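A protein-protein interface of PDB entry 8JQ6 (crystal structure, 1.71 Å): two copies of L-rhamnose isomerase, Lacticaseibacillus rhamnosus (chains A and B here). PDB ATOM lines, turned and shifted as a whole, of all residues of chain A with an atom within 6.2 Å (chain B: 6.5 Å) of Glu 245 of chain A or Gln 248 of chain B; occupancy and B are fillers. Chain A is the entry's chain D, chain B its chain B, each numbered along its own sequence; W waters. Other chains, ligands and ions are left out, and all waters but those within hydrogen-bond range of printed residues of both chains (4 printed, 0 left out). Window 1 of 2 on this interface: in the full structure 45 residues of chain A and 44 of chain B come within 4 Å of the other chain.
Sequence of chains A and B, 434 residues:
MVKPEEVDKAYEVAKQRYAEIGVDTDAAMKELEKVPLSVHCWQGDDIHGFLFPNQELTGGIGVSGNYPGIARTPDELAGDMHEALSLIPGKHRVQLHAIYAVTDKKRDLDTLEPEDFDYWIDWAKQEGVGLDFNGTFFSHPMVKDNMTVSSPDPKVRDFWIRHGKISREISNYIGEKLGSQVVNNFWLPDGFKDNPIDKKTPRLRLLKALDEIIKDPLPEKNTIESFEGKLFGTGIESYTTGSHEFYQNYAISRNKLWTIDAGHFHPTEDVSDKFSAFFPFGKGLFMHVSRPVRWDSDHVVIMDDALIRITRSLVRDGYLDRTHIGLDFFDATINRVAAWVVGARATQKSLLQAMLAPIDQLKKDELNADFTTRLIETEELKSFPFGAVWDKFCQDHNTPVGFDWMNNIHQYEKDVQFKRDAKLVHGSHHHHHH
Gln 248 of chain B touches two residues of chain A.
Of the printed residues of chain B, Gln 248 of chain A touches Glu 245 (3.5 Å) and Asn 249 (2.9 Å).
Of the printed residues of chain B, Asn 249 of chain A touches Gln 248, Asn 249, Ile 252, Ala 277 and Phe 281.
Printed residues of chain B within 4 Å of His 266 of chain A: Glu 269.
Printed residues of chain A within 4 Å of Lys 274 of chain B: Glu 245 (2.8 Å).
Trp 258 of chain B touches none of the printed residues of chain A.
Glu 245 of chain A touches Gln 248 of chain B (CG to NE2, 3.5 Å).
CB of Ala 277 of chain B touches N of Phe 246 of chain A, at 3.7 Å.
Phe 281 of chain B touches Phe 246 of chain A.
OD1 of Asn 249 of chain A touches OD1 of Asn 249 of chain B (3.998 Å).
Asn 249 of chain A touches Ile 252 of chain B (OD1 to CD1, 3.3 Å).
CE1 of Phe 281 of chain B touches CA of Tyr 250 of chain A (3.9 Å).
Glu 269 of chain B touches His 266 of chain A.
The side-chain amide oxygen (OE1) of Gln 248 of chain B lies within hydrogen-bond range of the side-chain amide nitrogen (ND2) of Asn 249 of chain A (2.9 Å).
The side-chain amide nitrogen (ND2) of Asn 249 of chain B lies within hydrogen-bond range of the side-chain amide oxygen (OE1) of Gln 248 of chain A (2.9 Å).
The side-chain amino group of Lys 274 of chain B is in salt-bridge range of the side-chain carboxylate of Glu 245 of chain A, at 2.8 Å.
O of Ala 277 of chain B sits at hydrogen-bond distance from ND2 of Asn 249 of chain A (3.0 Å).
Of the 21 printed residues of chain B, 8 touch a printed residue of chain A.
Glu 245 of chain A touches Gln 248 of chain B, and with the chains exchanged Gln 248 of chain A touches Glu 245 of chain B.
Asn 249 of chain B touches its own counterpart, Asn 249 of chain A.
9 positions are printed for both chains.
Of the 15 pairs that touch across the chains among the printed residues, 5 have their exchanged pair printed and touching as well.
ND2 of Asn 249 of chain B lies close to O of Glu 245 of chain B, 3.3 Å away.
OG of Ser 253 of chain B is in hydrogen-bond range of O of Asn 249 of chain B, at 2.9 Å.
OE1 of Glu 269 of chain B lies within salt-bridge range of NZ of Lys 274 of chain B.
O of Glu 245 of chain A sits close to ND2 of Asn 249 of chain A (3.2 Å).
Water W3 lies within hydrogen-bond range of OD1 of Asn 249 of chain A and OD1 of Asn 249 of chain B.
Water W1 lies within hydrogen-bond range of OG of Ser 243 of chain A, OD2 of Asp 273 of chain B and OE1 of Glu 245 of chain A.
Water W2 bridges OD1 of Asn 249 of chain B (2.8 Å) and OD1 of Asn 249 of chain A (2.9 Å).
Water W4 bridges the side-chain amide nitrogen of Gln 248 of chain B and the side-chain amide nitrogen of Gln 248 of chain A.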
ATOM      1  N   SER A 243     -12.519   9.222  13.164  1.00  0.00           N
ATOM      2  CA  SER A 243     -11.567   8.104  12.948  1.00  0.00           C
ATOM      3  C   SER A 243     -11.603   7.137  14.136  1.00  0.00           C
ATOM      4  O   SER A 243     -12.151   7.491  15.213  1.00  0.00           O
ATOM      5  CB  SER A 243     -10.175   8.622  12.711  1.00  0.00           C
ATOM      6  OG  SER A 243      -9.646   9.159  13.912  1.00  0.00           O
ATOM      7  N   HIS A 244     -11.011   5.961  13.961  1.00  0.00           N
ATOM      8  CA  HIS A 244     -10.880   4.941  15.026  1.00  0.00           C
ATOM      9  C   HIS A 244     -10.088   5.542  16.191  1.00  0.00           C
ATOM     10  O   HIS A 244     -10.473   5.323  17.347  1.00  0.00           O
ATOM     11  CB  HIS A 244     -10.240   3.669  14.484  1.00  0.00           C
ATOM     12  CG  HIS A 244     -11.025   3.013  13.399  1.00  0.00           C
ATOM     13  ND1 HIS A 244     -12.346   2.647  13.568  1.00  0.00           N
ATOM     14  CD2 HIS A 244     -10.670   2.634  12.153  1.00  0.00           C
ATOM     15  CE1 HIS A 244     -12.780   2.068  12.471  1.00  0.00           C
ATOM     16  NE2 HIS A 244     -11.769   2.056  11.571  1.00  0.00           N
ATOM     17  N   GLU A 245      -9.018   6.276  15.901  1.00  0.00           N
ATOM     18  CA  GLU A 245      -8.174   6.915  16.948  1.00  0.00           C
ATOM     19  C   GLU A 245      -9.011   7.952  17.701  1.00  0.00           C
ATOM     20  O   GLU A 245      -8.979   7.972  18.956  1.00  0.00           O
ATOM     21  CB  GLU A 245      -6.937   7.563  16.333  1.00  0.00           C
ATOM     22  CG  GLU A 245      -5.888   6.557  15.879  1.00  0.00           C
ATOM     23  CD  GLU A 245      -6.154   5.899  14.531  1.00  0.00           C
ATOM     24  OE1 GLU A 245      -7.082   6.336  13.795  1.00  0.00           O
ATOM     25  OE2 GLU A 245      -5.422   4.954  14.216  1.00  0.00           O
ATOM     26  N   PHE A 246      -9.739   8.784  16.966  1.00  0.00           N
ATOM     27  CA  PHE A 246     -10.553   9.861  17.573  1.00  0.00           C
ATOM     28  C   PHE A 246     -11.513   9.219  18.578  1.00  0.00           C
ATOM     29  O   PHE A 246     -11.595   9.642  19.733  1.00  0.00           O
ATOM     30  CB  PHE A 246     -11.309  10.664  16.519  1.00  0.00           C
ATOM     31  CG  PHE A 246     -12.188  11.725  17.128  1.00  0.00           C
ATOM     32  CD1 PHE A 246     -11.685  12.989  17.373  1.00  0.00           C
ATOM     33  CD2 PHE A 246     -13.479  11.433  17.540  1.00  0.00           C
ATOM     34  CE1 PHE A 246     -12.475  13.966  17.948  1.00  0.00           C
ATOM     35  CE2 PHE A 246     -14.269  12.404  18.129  1.00  0.00           C
ATOM     36  CZ  PHE A 246     -13.760  13.672  18.330  1.00  0.00           C
ATOM     37  N   TYR A 247     -12.228   8.185  18.153  1.00  0.00           N
ATOM     38  CA  TYR A 247     -13.324   7.612  18.971  1.00  0.00           C
ATOM     39  C   TYR A 247     -12.762   6.730  20.087  1.00  0.00           C
ATOM     40  O   TYR A 247     -13.393   6.701  21.159  1.00  0.00           O
ATOM     41  CB  TYR A 247     -14.304   6.860  18.078  1.00  0.00           C
ATOM     42  CG  TYR A 247     -15.250   7.724  17.283  1.00  0.00           C
ATOM     43  CD1 TYR A 247     -15.994   8.728  17.882  1.00  0.00           C
ATOM     44  CD2 TYR A 247     -15.481   7.463  15.940  1.00  0.00           C
ATOM     45  CE1 TYR A 247     -16.917   9.469  17.165  1.00  0.00           C
ATOM     46  CE2 TYR A 247     -16.401   8.190  15.208  1.00  0.00           C
ATOM     47  CZ  TYR A 247     -17.127   9.194  15.823  1.00  0.00           C
ATOM     48  OH  TYR A 247     -18.035   9.913  15.109  1.00  0.00           O
ATOM     49  N   GLN A 248     -11.641   6.026  19.888  1.00  0.00           N
ATOM     50  CA  GLN A 248     -11.039   5.280  21.025  1.00  0.00           C
ATOM     51  C   GLN A 248     -10.638   6.304  22.098  1.00  0.00           C
ATOM     52  O   GLN A 248     -10.935   6.093  23.284  1.00  0.00           O
ATOM     53  CB  GLN A 248      -9.861   4.390  20.620  1.00  0.00           C
ATOM     54  CG  GLN A 248      -9.279   3.674  21.833  1.00  0.00           C
ATOM     55  CD  GLN A 248      -8.406   2.464  21.608  1.00  0.00           C
ATOM     56  OE1 GLN A 248      -8.095   1.746  22.562  1.00  0.00           O
ATOM     57  NE2 GLN A 248      -7.983   2.232  20.370  1.00  0.00           N
ATOM     58  N   ASN A 249      -9.994   7.390  21.683  1.00  0.00           N
ATOM     59  CA  ASN A 249      -9.599   8.487  22.602  1.00  0.00           C
ATOM     60  C   ASN A 249     -10.854   9.063  23.262  1.00  0.00           C
ATOM     61  O   ASN A 249     -10.824   9.339  24.486  1.00  0.00           O
ATOM     62  CB  ASN A 249      -8.822   9.586  21.878  1.00  0.00           C
ATOM     63  CG  ASN A 249      -7.445   9.137  21.446  1.00  0.00           C
ATOM     64  OD1 ASN A 249      -6.919   8.165  21.979  1.00  0.00           O
ATOM     65  ND2 ASN A 249      -6.847   9.860  20.506  1.00  0.00           N
ATOM     66  N   TYR A 250     -11.911   9.278  22.481  1.00  0.00           N
ATOM     67  CA  TYR A 250     -13.130   9.957  22.978  1.00  0.00           C
ATOM     68  C   TYR A 250     -13.804   9.051  24.008  1.00  0.00           C
ATOM     69  O   TYR A 250     -14.158   9.541  25.107  1.00  0.00           O
ATOM     70  CB  TYR A 250     -14.073  10.340  21.835  1.00  0.00           C
ATOM     71  CG  TYR A 250     -15.235  11.158  22.327  1.00  0.00           C
ATOM     72  CD1 TYR A 250     -15.102  12.517  22.553  1.00  0.00           C
ATOM     73  CD2 TYR A 250     -16.437  10.560  22.661  1.00  0.00           C
ATOM     74  CE1 TYR A 250     -16.152  13.273  23.046  1.00  0.00           C
ATOM     75  CE2 TYR A 250     -17.500  11.300  23.149  1.00  0.00           C
ATOM     76  CZ  TYR A 250     -17.355  12.663  23.353  1.00  0.00           C
ATOM     77  OH  TYR A 250     -18.387  13.409  23.847  1.00  0.00           O
ATOM     78  N   TRP A 258     -16.585   2.080  23.014  1.00  0.00           N
ATOM     79  CA  TRP A 258     -15.977   2.197  21.671  1.00  0.00           C
ATOM     80  C   TRP A 258     -16.536   1.091  20.773  1.00  0.00           C
ATOM     81  O   TRP A 258     -16.540  -0.076  21.197  1.00  0.00           O
ATOM     82  CB  TRP A 258     -14.458   2.142  21.808  1.00  0.00           C
ATOM     83  CG  TRP A 258     -13.734   2.314  20.512  1.00  0.00           C
ATOM     84  CD1 TRP A 258     -14.064   3.138  19.473  1.00  0.00           C
ATOM     85  CD2 TRP A 258     -12.552   1.607  20.111  1.00  0.00           C
ATOM     86  NE1 TRP A 258     -13.160   2.999  18.458  1.00  0.00           N
ATOM     87  CE2 TRP A 258     -12.227   2.060  18.817  1.00  0.00           C
ATOM     88  CE3 TRP A 258     -11.743   0.638  20.718  1.00  0.00           C
ATOM     89  CZ2 TRP A 258     -11.119   1.567  18.125  1.00  0.00           C
ATOM     90  CZ3 TRP A 258     -10.649   0.160  20.033  1.00  0.00           C
ATOM     91  CH2 TRP A 258     -10.344   0.621  18.753  1.00  0.00           C
ATOM     92  N   HIS A 266      -8.043  -1.049   7.886  1.00  0.00           N
ATOM     93  CA  HIS A 266      -7.096  -1.132   6.742  1.00  0.00           C
ATOM     94  C   HIS A 266      -7.074  -2.546   6.176  1.00  0.00           C
ATOM     95  O   HIS A 266      -7.400  -3.516   6.848  1.00  0.00           O
ATOM     96  CB  HIS A 266      -5.688  -0.714   7.159  1.00  0.00           C
ATOM     97  CG  HIS A 266      -5.568   0.736   7.466  1.00  0.00           C
ATOM     98  ND1 HIS A 266      -5.829   1.243   8.722  1.00  0.00           N
ATOM     99  CD2 HIS A 266      -5.228   1.787   6.685  1.00  0.00           C
ATOM    100  CE1 HIS A 266      -5.657   2.555   8.700  1.00  0.00           C
ATOM    101  NE2 HIS A 266      -5.290   2.914   7.463  1.00  0.00           N
ATOM    102  N   PHE B 227       6.772   7.142  23.468  1.00  0.00           N
ATOM    103  CA  PHE B 227       6.546   5.681  23.392  1.00  0.00           C
ATOM    104  C   PHE B 227       6.206   5.298  21.959  1.00  0.00           C
ATOM    105  O   PHE B 227       5.244   5.830  21.388  1.00  0.00           O
ATOM    106  CB  PHE B 227       5.494   5.271  24.417  1.00  0.00           C
ATOM    107  CG  PHE B 227       5.958   5.564  25.820  1.00  0.00           C
ATOM    108  CD1 PHE B 227       6.748   4.653  26.496  1.00  0.00           C
ATOM    109  CD2 PHE B 227       5.669   6.774  26.433  1.00  0.00           C
ATOM    110  CE1 PHE B 227       7.219   4.923  27.768  1.00  0.00           C
ATOM    111  CE2 PHE B 227       6.136   7.045  27.711  1.00  0.00           C
ATOM    112  CZ  PHE B 227       6.908   6.121  28.376  1.00  0.00           C
ATOM    113  N   SER B 243       1.559  -1.979  21.029  1.00  0.00           N
ATOM    114  CA  SER B 243       0.828  -1.616  19.790  1.00  0.00           C
ATOM    115  C   SER B 243       0.670  -0.096  19.726  1.00  0.00           C
ATOM    116  O   SER B 243       0.845   0.594  20.782  1.00  0.00           O
ATOM    117  CB  SER B 243      -0.505  -2.326  19.697  1.00  0.00           C
ATOM    118  OG  SER B 243      -1.403  -1.850  20.691  1.00  0.00           O
ATOM    119  N   HIS B 244       0.321   0.422  18.552  1.00  0.00           N
ATOM    120  CA  HIS B 244       0.022   1.862  18.353  1.00  0.00           C
ATOM    121  C   HIS B 244      -1.132   2.281  19.265  1.00  0.00           C
ATOM    122  O   HIS B 244      -1.070   3.385  19.815  1.00  0.00           O
ATOM    123  CB  HIS B 244      -0.294   2.152  16.887  1.00  0.00           C
ATOM    124  CG  HIS B 244       0.846   1.849  15.989  1.00  0.00           C
ATOM    125  ND1 HIS B 244       2.101   2.386  16.185  1.00  0.00           N
ATOM    126  CD2 HIS B 244       0.931   1.040  14.916  1.00  0.00           C
ATOM    127  CE1 HIS B 244       2.911   1.932  15.251  1.00  0.00           C
ATOM    128  NE2 HIS B 244       2.217   1.100  14.462  1.00  0.00           N
ATOM    129  N   GLU B 245      -2.174   1.457  19.378  1.00  0.00           N
ATOM    130  CA  GLU B 245      -3.340   1.775  20.242  1.00  0.00           C
ATOM    131  C   GLU B 245      -2.866   1.825  21.695  1.00  0.00           C
ATOM    132  O   GLU B 245      -3.184   2.802  22.408  1.00  0.00           O
ATOM    133  CB  GLU B 245      -4.446   0.734  20.068  1.00  0.00           C
ATOM    134  CG  GLU B 245      -5.190   0.849  18.749  1.00  0.00           C
ATOM    135  CD  GLU B 245      -4.480   0.251  17.544  1.00  0.00           C
ATOM    136  OE1 GLU B 245      -3.428  -0.421  17.728  1.00  0.00           O
ATOM    137  OE2 GLU B 245      -4.989   0.450  16.418  1.00  0.00           O
ATOM    138  N   PHE B 246      -2.116   0.811  22.124  1.00  0.00           N
ATOM    139  CA  PHE B 246      -1.639   0.719  23.518  1.00  0.00           C
ATOM    140  C   PHE B 246      -0.869   2.005  23.866  1.00  0.00           C
ATOM    141  O   PHE B 246      -1.101   2.608  24.921  1.00  0.00           O
ATOM    142  CB  PHE B 246      -0.770  -0.518  23.737  1.00  0.00           C
ATOM    143  CG  PHE B 246      -0.215  -0.565  25.135  1.00  0.00           C
ATOM    144  CD1 PHE B 246      -0.890  -1.237  26.140  1.00  0.00           C
ATOM    145  CD2 PHE B 246       0.922   0.149  25.465  1.00  0.00           C
ATOM    146  CE1 PHE B 246      -0.394  -1.253  27.435  1.00  0.00           C
ATOM    147  CE2 PHE B 246       1.406   0.144  26.764  1.00  0.00           C
ATOM    148  CZ  PHE B 246       0.747  -0.556  27.746  1.00  0.00           C
ATOM    149  N   TYR B 247       0.043   2.445  23.003  1.00  0.00           N
ATOM    150  CA  TYR B 247       0.927   3.577  23.362  1.00  0.00           C
ATOM    151  C   TYR B 247       0.208   4.918  23.220  1.00  0.00           C
ATOM    152  O   TYR B 247       0.563   5.832  23.983  1.00  0.00           O
ATOM    153  CB  TYR B 247       2.211   3.559  22.542  1.00  0.00           C
ATOM    154  CG  TYR B 247       3.224   2.537  22.982  1.00  0.00           C
ATOM    155  CD1 TYR B 247       3.655   2.469  24.294  1.00  0.00           C
ATOM    156  CD2 TYR B 247       3.786   1.659  22.070  1.00  0.00           C
ATOM    157  CE1 TYR B 247       4.623   1.563  24.689  1.00  0.00           C
ATOM    158  CE2 TYR B 247       4.749   0.739  22.450  1.00  0.00           C
ATOM    159  CZ  TYR B 247       5.174   0.695  23.762  1.00  0.00           C
ATOM    160  OH  TYR B 247       6.147  -0.176  24.143  1.00  0.00           O
ATOM    161  N   GLN B 248      -0.709   5.084  22.266  1.00  0.00           N
ATOM    162  CA  GLN B 248      -1.486   6.346  22.184  1.00  0.00           C
ATOM    163  C   GLN B 248      -2.299   6.466  23.480  1.00  0.00           C
ATOM    164  O   GLN B 248      -2.298   7.560  24.113  1.00  0.00           O
ATOM    165  CB  GLN B 248      -2.375   6.425  20.940  1.00  0.00           C
ATOM    166  CG  GLN B 248      -3.162   7.727  20.907  1.00  0.00           C
ATOM    167  CD  GLN B 248      -3.782   8.170  19.607  1.00  0.00           C
ATOM    168  OE1 GLN B 248      -4.226   9.312  19.505  1.00  0.00           O
ATOM    169  NE2 GLN B 248      -3.842   7.282  18.616  1.00  0.00           N
ATOM    170  N   ASN B 249      -2.928   5.373  23.904  1.00  0.00           N
ATOM    171  CA  ASN B 249      -3.688   5.344  25.179  1.00  0.00           C
ATOM    172  C   ASN B 249      -2.732   5.643  26.339  1.00  0.00           C
ATOM    173  O   ASN B 249      -3.101   6.419  27.263  1.00  0.00           O
ATOM    174  CB  ASN B 249      -4.403   4.015  25.405  1.00  0.00           C
ATOM    175  CG  ASN B 249      -5.524   3.780  24.415  1.00  0.00           C
ATOM    176  OD1 ASN B 249      -6.049   4.722  23.815  1.00  0.00           O
ATOM    177  ND2 ASN B 249      -5.895   2.524  24.239  1.00  0.00           N
ATOM    178  N   TYR B 250      -1.558   5.027  26.334  1.00  0.00           N
ATOM    179  CA  TYR B 250      -0.596   5.157  27.457  1.00  0.00           C
ATOM    180  C   TYR B 250      -0.101   6.606  27.526  1.00  0.00           C
ATOM    181  O   TYR B 250      -0.082   7.198  28.624  1.00  0.00           O
ATOM    182  CB  TYR B 250       0.559   4.164  27.335  1.00  0.00           C
ATOM    183  CG  TYR B 250       1.431   4.185  28.555  1.00  0.00           C
ATOM    184  CD1 TYR B 250       1.072   3.477  29.684  1.00  0.00           C
ATOM    185  CD2 TYR B 250       2.580   4.959  28.605  1.00  0.00           C
ATOM    186  CE1 TYR B 250       1.844   3.510  30.831  1.00  0.00           C
ATOM    187  CE2 TYR B 250       3.369   4.994  29.743  1.00  0.00           C
ATOM    188  CZ  TYR B 250       2.990   4.280  30.868  1.00  0.00           C
ATOM    189  OH  TYR B 250       3.751   4.312  32.001  1.00  0.00           O
ATOM    190  N   ALA B 251       0.283   7.182  26.388  1.00  0.00           N
ATOM    191  CA  ALA B 251       0.794   8.573  26.327  1.00  0.00           C
ATOM    192  C   ALA B 251      -0.274   9.526  26.882  1.00  0.00           C
ATOM    193  O   ALA B 251       0.029  10.346  27.788  1.00  0.00           O
ATOM    194  CB  ALA B 251       1.178   8.920  24.910  1.00  0.00           C
ATOM    195  N   ILE B 252      -1.499   9.428  26.375  1.00  0.00           N
ATOM    196  CA  ILE B 252      -2.603  10.334  26.790  1.00  0.00           C
ATOM    197  C   ILE B 252      -2.834  10.169  28.299  1.00  0.00           C
ATOM    198  O   ILE B 252      -2.933  11.196  28.994  1.00  0.00           O
ATOM    199  CB  ILE B 252      -3.876  10.078  25.961  1.00  0.00           C
ATOM    200  CG1 ILE B 252      -3.701  10.558  24.520  1.00  0.00           C
ATOM    201  CG2 ILE B 252      -5.085  10.723  26.622  1.00  0.00           C
ATOM    202  CD1 ILE B 252      -4.739  10.044  23.558  1.00  0.00           C
ATOM    203  N   SER B 253      -2.885   8.942  28.816  1.00  0.00           N
ATOM    204  CA  SER B 253      -3.280   8.711  30.233  1.00  0.00           C
ATOM    205  C   SER B 253      -2.133   9.097  31.181  1.00  0.00           C
ATOM    206  O   SER B 253      -2.441   9.546  32.293  1.00  0.00           O
ATOM    207  CB  SER B 253      -3.799   7.311  30.493  1.00  0.00           C
ATOM    208  OG  SER B 253      -2.829   6.341  30.183  1.00  0.00           O
ATOM    209  N   TRP B 258       3.735  10.552  22.293  1.00  0.00           N
ATOM    210  CA  TRP B 258       3.454   9.379  21.441  1.00  0.00           C
ATOM    211  C   TRP B 258       4.376   9.447  20.226  1.00  0.00           C
ATOM    212  O   TRP B 258       4.443  10.518  19.589  1.00  0.00           O
ATOM    213  CB  TRP B 258       1.970   9.330  21.071  1.00  0.00           C
ATOM    214  CG  TRP B 258       1.600   8.130  20.251  1.00  0.00           C
ATOM    215  CD1 TRP B 258       2.077   6.858  20.390  1.00  0.00           C
ATOM    216  CD2 TRP B 258       0.657   8.086  19.167  1.00  0.00           C
ATOM    217  NE1 TRP B 258       1.519   6.028  19.450  1.00  0.00           N
ATOM    218  CE2 TRP B 258       0.636   6.752  18.691  1.00  0.00           C
ATOM    219  CE3 TRP B 258      -0.161   9.038  18.551  1.00  0.00           C
ATOM    220  CZ2 TRP B 258      -0.163   6.361  17.623  1.00  0.00           C
ATOM    221  CZ3 TRP B 258      -0.967   8.644  17.508  1.00  0.00           C
ATOM    222  CH2 TRP B 258      -0.953   7.329  17.041  1.00  0.00           C
ATOM    223  N   PHE B 265       3.260   0.964  10.249  1.00  0.00           N
ATOM    224  CA  PHE B 265       1.779   0.847  10.164  1.00  0.00           C
ATOM    225  C   PHE B 265       1.360  -0.139   9.062  1.00  0.00           C
ATOM    226  O   PHE B 265       2.207  -0.859   8.479  1.00  0.00           O
ATOM    227  CB  PHE B 265       1.169   2.245  10.028  1.00  0.00           C
ATOM    228  CG  PHE B 265       1.291   3.058  11.293  1.00  0.00           C
ATOM    229  CD1 PHE B 265       0.227   3.190  12.170  1.00  0.00           C
ATOM    230  CD2 PHE B 265       2.492   3.658  11.628  1.00  0.00           C
ATOM    231  CE1 PHE B 265       0.364   3.915  13.345  1.00  0.00           C
ATOM    232  CE2 PHE B 265       2.620   4.392  12.797  1.00  0.00           C
ATOM    233  CZ  PHE B 265       1.554   4.523  13.652  1.00  0.00           C
ATOM    234  N   GLU B 269      -1.772   2.601   5.075  1.00  0.00           N
ATOM    235  CA  GLU B 269      -2.121   3.422   6.261  1.00  0.00           C
ATOM    236  C   GLU B 269      -1.419   4.780   6.138  1.00  0.00           C
ATOM    237  O   GLU B 269      -0.215   4.808   5.839  1.00  0.00           O
ATOM    238  CB  GLU B 269      -1.791   2.665   7.547  1.00  0.00           C
ATOM    239  CG  GLU B 269      -2.260   3.376   8.806  1.00  0.00           C
ATOM    240  CD  GLU B 269      -2.503   2.454   9.987  1.00  0.00           C
ATOM    241  OE1 GLU B 269      -3.224   2.869  10.933  1.00  0.00           O
ATOM    242  OE2 GLU B 269      -1.979   1.327   9.961  1.00  0.00           O
ATOM    243  N   ASP B 273      -2.929  11.081   9.080  1.00  0.00           N
ATOM    244  CA  ASP B 273      -4.328  11.104   9.583  1.00  0.00           C
ATOM    245  C   ASP B 273      -4.336  11.192  11.114  1.00  0.00           C
ATOM    246  O   ASP B 273      -5.351  11.667  11.679  1.00  0.00           O
ATOM    247  CB  ASP B 273      -5.088   9.853   9.144  1.00  0.00           C
ATOM    248  CG  ASP B 273      -6.558   9.866   9.524  1.00  0.00           C
ATOM    249  OD1 ASP B 273      -7.262  10.805   9.092  1.00  0.00           O
ATOM    250  OD2 ASP B 273      -6.986   8.938  10.256  1.00  0.00           O
ATOM    251  N   LYS B 274      -3.274  10.730  11.781  1.00  0.00           N
ATOM    252  CA  LYS B 274      -3.311  10.475  13.249  1.00  0.00           C
ATOM    253  C   LYS B 274      -3.227  11.795  14.032  1.00  0.00           C
ATOM    254  O   LYS B 274      -3.787  11.866  15.134  1.00  0.00           O
ATOM    255  CB  LYS B 274      -2.179   9.549  13.716  1.00  0.00           C
ATOM    256  CG  LYS B 274      -2.020   8.226  12.975  1.00  0.00           C
ATOM    257  CD  LYS B 274      -3.270   7.411  12.796  1.00  0.00           C
ATOM    258  CE  LYS B 274      -2.957   6.100  12.089  1.00  0.00           C
ATOM    259  NZ  LYS B 274      -4.162   5.303  11.793  1.00  0.00           N
ATOM    260  N   ALA B 277      -6.411  13.534  15.325  1.00  0.00           N
ATOM    261  CA  ALA B 277      -7.195  12.640  16.216  1.00  0.00           C
ATOM    262  C   ALA B 277      -6.507  12.552  17.583  1.00  0.00           C
ATOM    263  O   ALA B 277      -7.162  12.184  18.568  1.00  0.00           O
ATOM    264  CB  ALA B 277      -7.345  11.272  15.579  1.00  0.00           C
ATOM    265  N   PHE B 278      -5.219  12.898  17.646  1.00  0.00           N
ATOM    266  CA  PHE B 278      -4.402  12.813  18.883  1.00  0.00           C
ATOM    267  C   PHE B 278      -4.490  14.125  19.669  1.00  0.00           C
ATOM    268  O   PHE B 278      -4.712  14.096  20.900  1.00  0.00           O
ATOM    269  CB  PHE B 278      -2.945  12.506  18.549  1.00  0.00           C
ATOM    270  CG  PHE B 278      -2.016  12.598  19.728  1.00  0.00           C
ATOM    271  CD1 PHE B 278      -1.922  11.557  20.641  1.00  0.00           C
ATOM    272  CD2 PHE B 278      -1.235  13.729  19.925  1.00  0.00           C
ATOM    273  CE1 PHE B 278      -1.065  11.640  21.725  1.00  0.00           C
ATOM    274  CE2 PHE B 278      -0.381  13.813  21.014  1.00  0.00           C
ATOM    275  CZ  PHE B 278      -0.291  12.769  21.908  1.00  0.00           C
ATOM    276  N   PHE B 279      -4.318  15.258  18.997  1.00  0.00           N
ATOM    277  CA  PHE B 279      -4.045  16.541  19.695  1.00  0.00           C
ATOM    278  C   PHE B 279      -5.257  17.080  20.461  1.00  0.00           C
ATOM    279  O   PHE B 279      -5.071  17.915  21.345  1.00  0.00           O
ATOM    280  CB  PHE B 279      -3.430  17.548  18.725  1.00  0.00           C
ATOM    281  CG  PHE B 279      -1.936  17.397  18.599  1.00  0.00           C
ATOM    282  CD1 PHE B 279      -1.127  17.473  19.723  1.00  0.00           C
ATOM    283  CD2 PHE B 279      -1.341  17.162  17.369  1.00  0.00           C
ATOM    284  CE1 PHE B 279       0.246  17.339  19.622  1.00  0.00           C
ATOM    285  CE2 PHE B 279       0.038  17.040  17.271  1.00  0.00           C
ATOM    286  CZ  PHE B 279       0.827  17.122  18.393  1.00  0.00           C
ATOM    287  N   PHE B 281      -6.588  15.451  22.663  1.00  0.00           N
ATOM    288  CA  PHE B 281      -6.499  14.623  23.896  1.00  0.00           C
ATOM    289  C   PHE B 281      -5.083  14.628  24.478  1.00  0.00           C
ATOM    290  O   PHE B 281      -4.955  14.571  25.722  1.00  0.00           O
ATOM    291  CB  PHE B 281      -6.959  13.193  23.600  1.00  0.00           C
ATOM    292  CG  PHE B 281      -8.285  13.100  22.893  1.00  0.00           C
ATOM    293  CD1 PHE B 281      -9.471  13.105  23.612  1.00  0.00           C
ATOM    294  CD2 PHE B 281      -8.345  12.998  21.510  1.00  0.00           C
ATOM    295  CE1 PHE B 281     -10.689  12.990  22.962  1.00  0.00           C
ATOM    296  CE2 PHE B 281      -9.564  12.886  20.861  1.00  0.00           C
ATOM    297  CZ  PHE B 281     -10.735  12.885  21.592  1.00  0.00           C
HETATM  298  O   HOH W   1      -7.023   9.059  13.042  1.00  0.00           O
HETATM  299  O   HOH W   2      -6.772   7.314  24.704  1.00  0.00           O
HETATM  300  O   HOH W   3      -6.187   5.671  21.159  1.00  0.00           O
HETATM  301  O   HOH W   4      -5.770   4.398  18.750  1.00  0.00           O
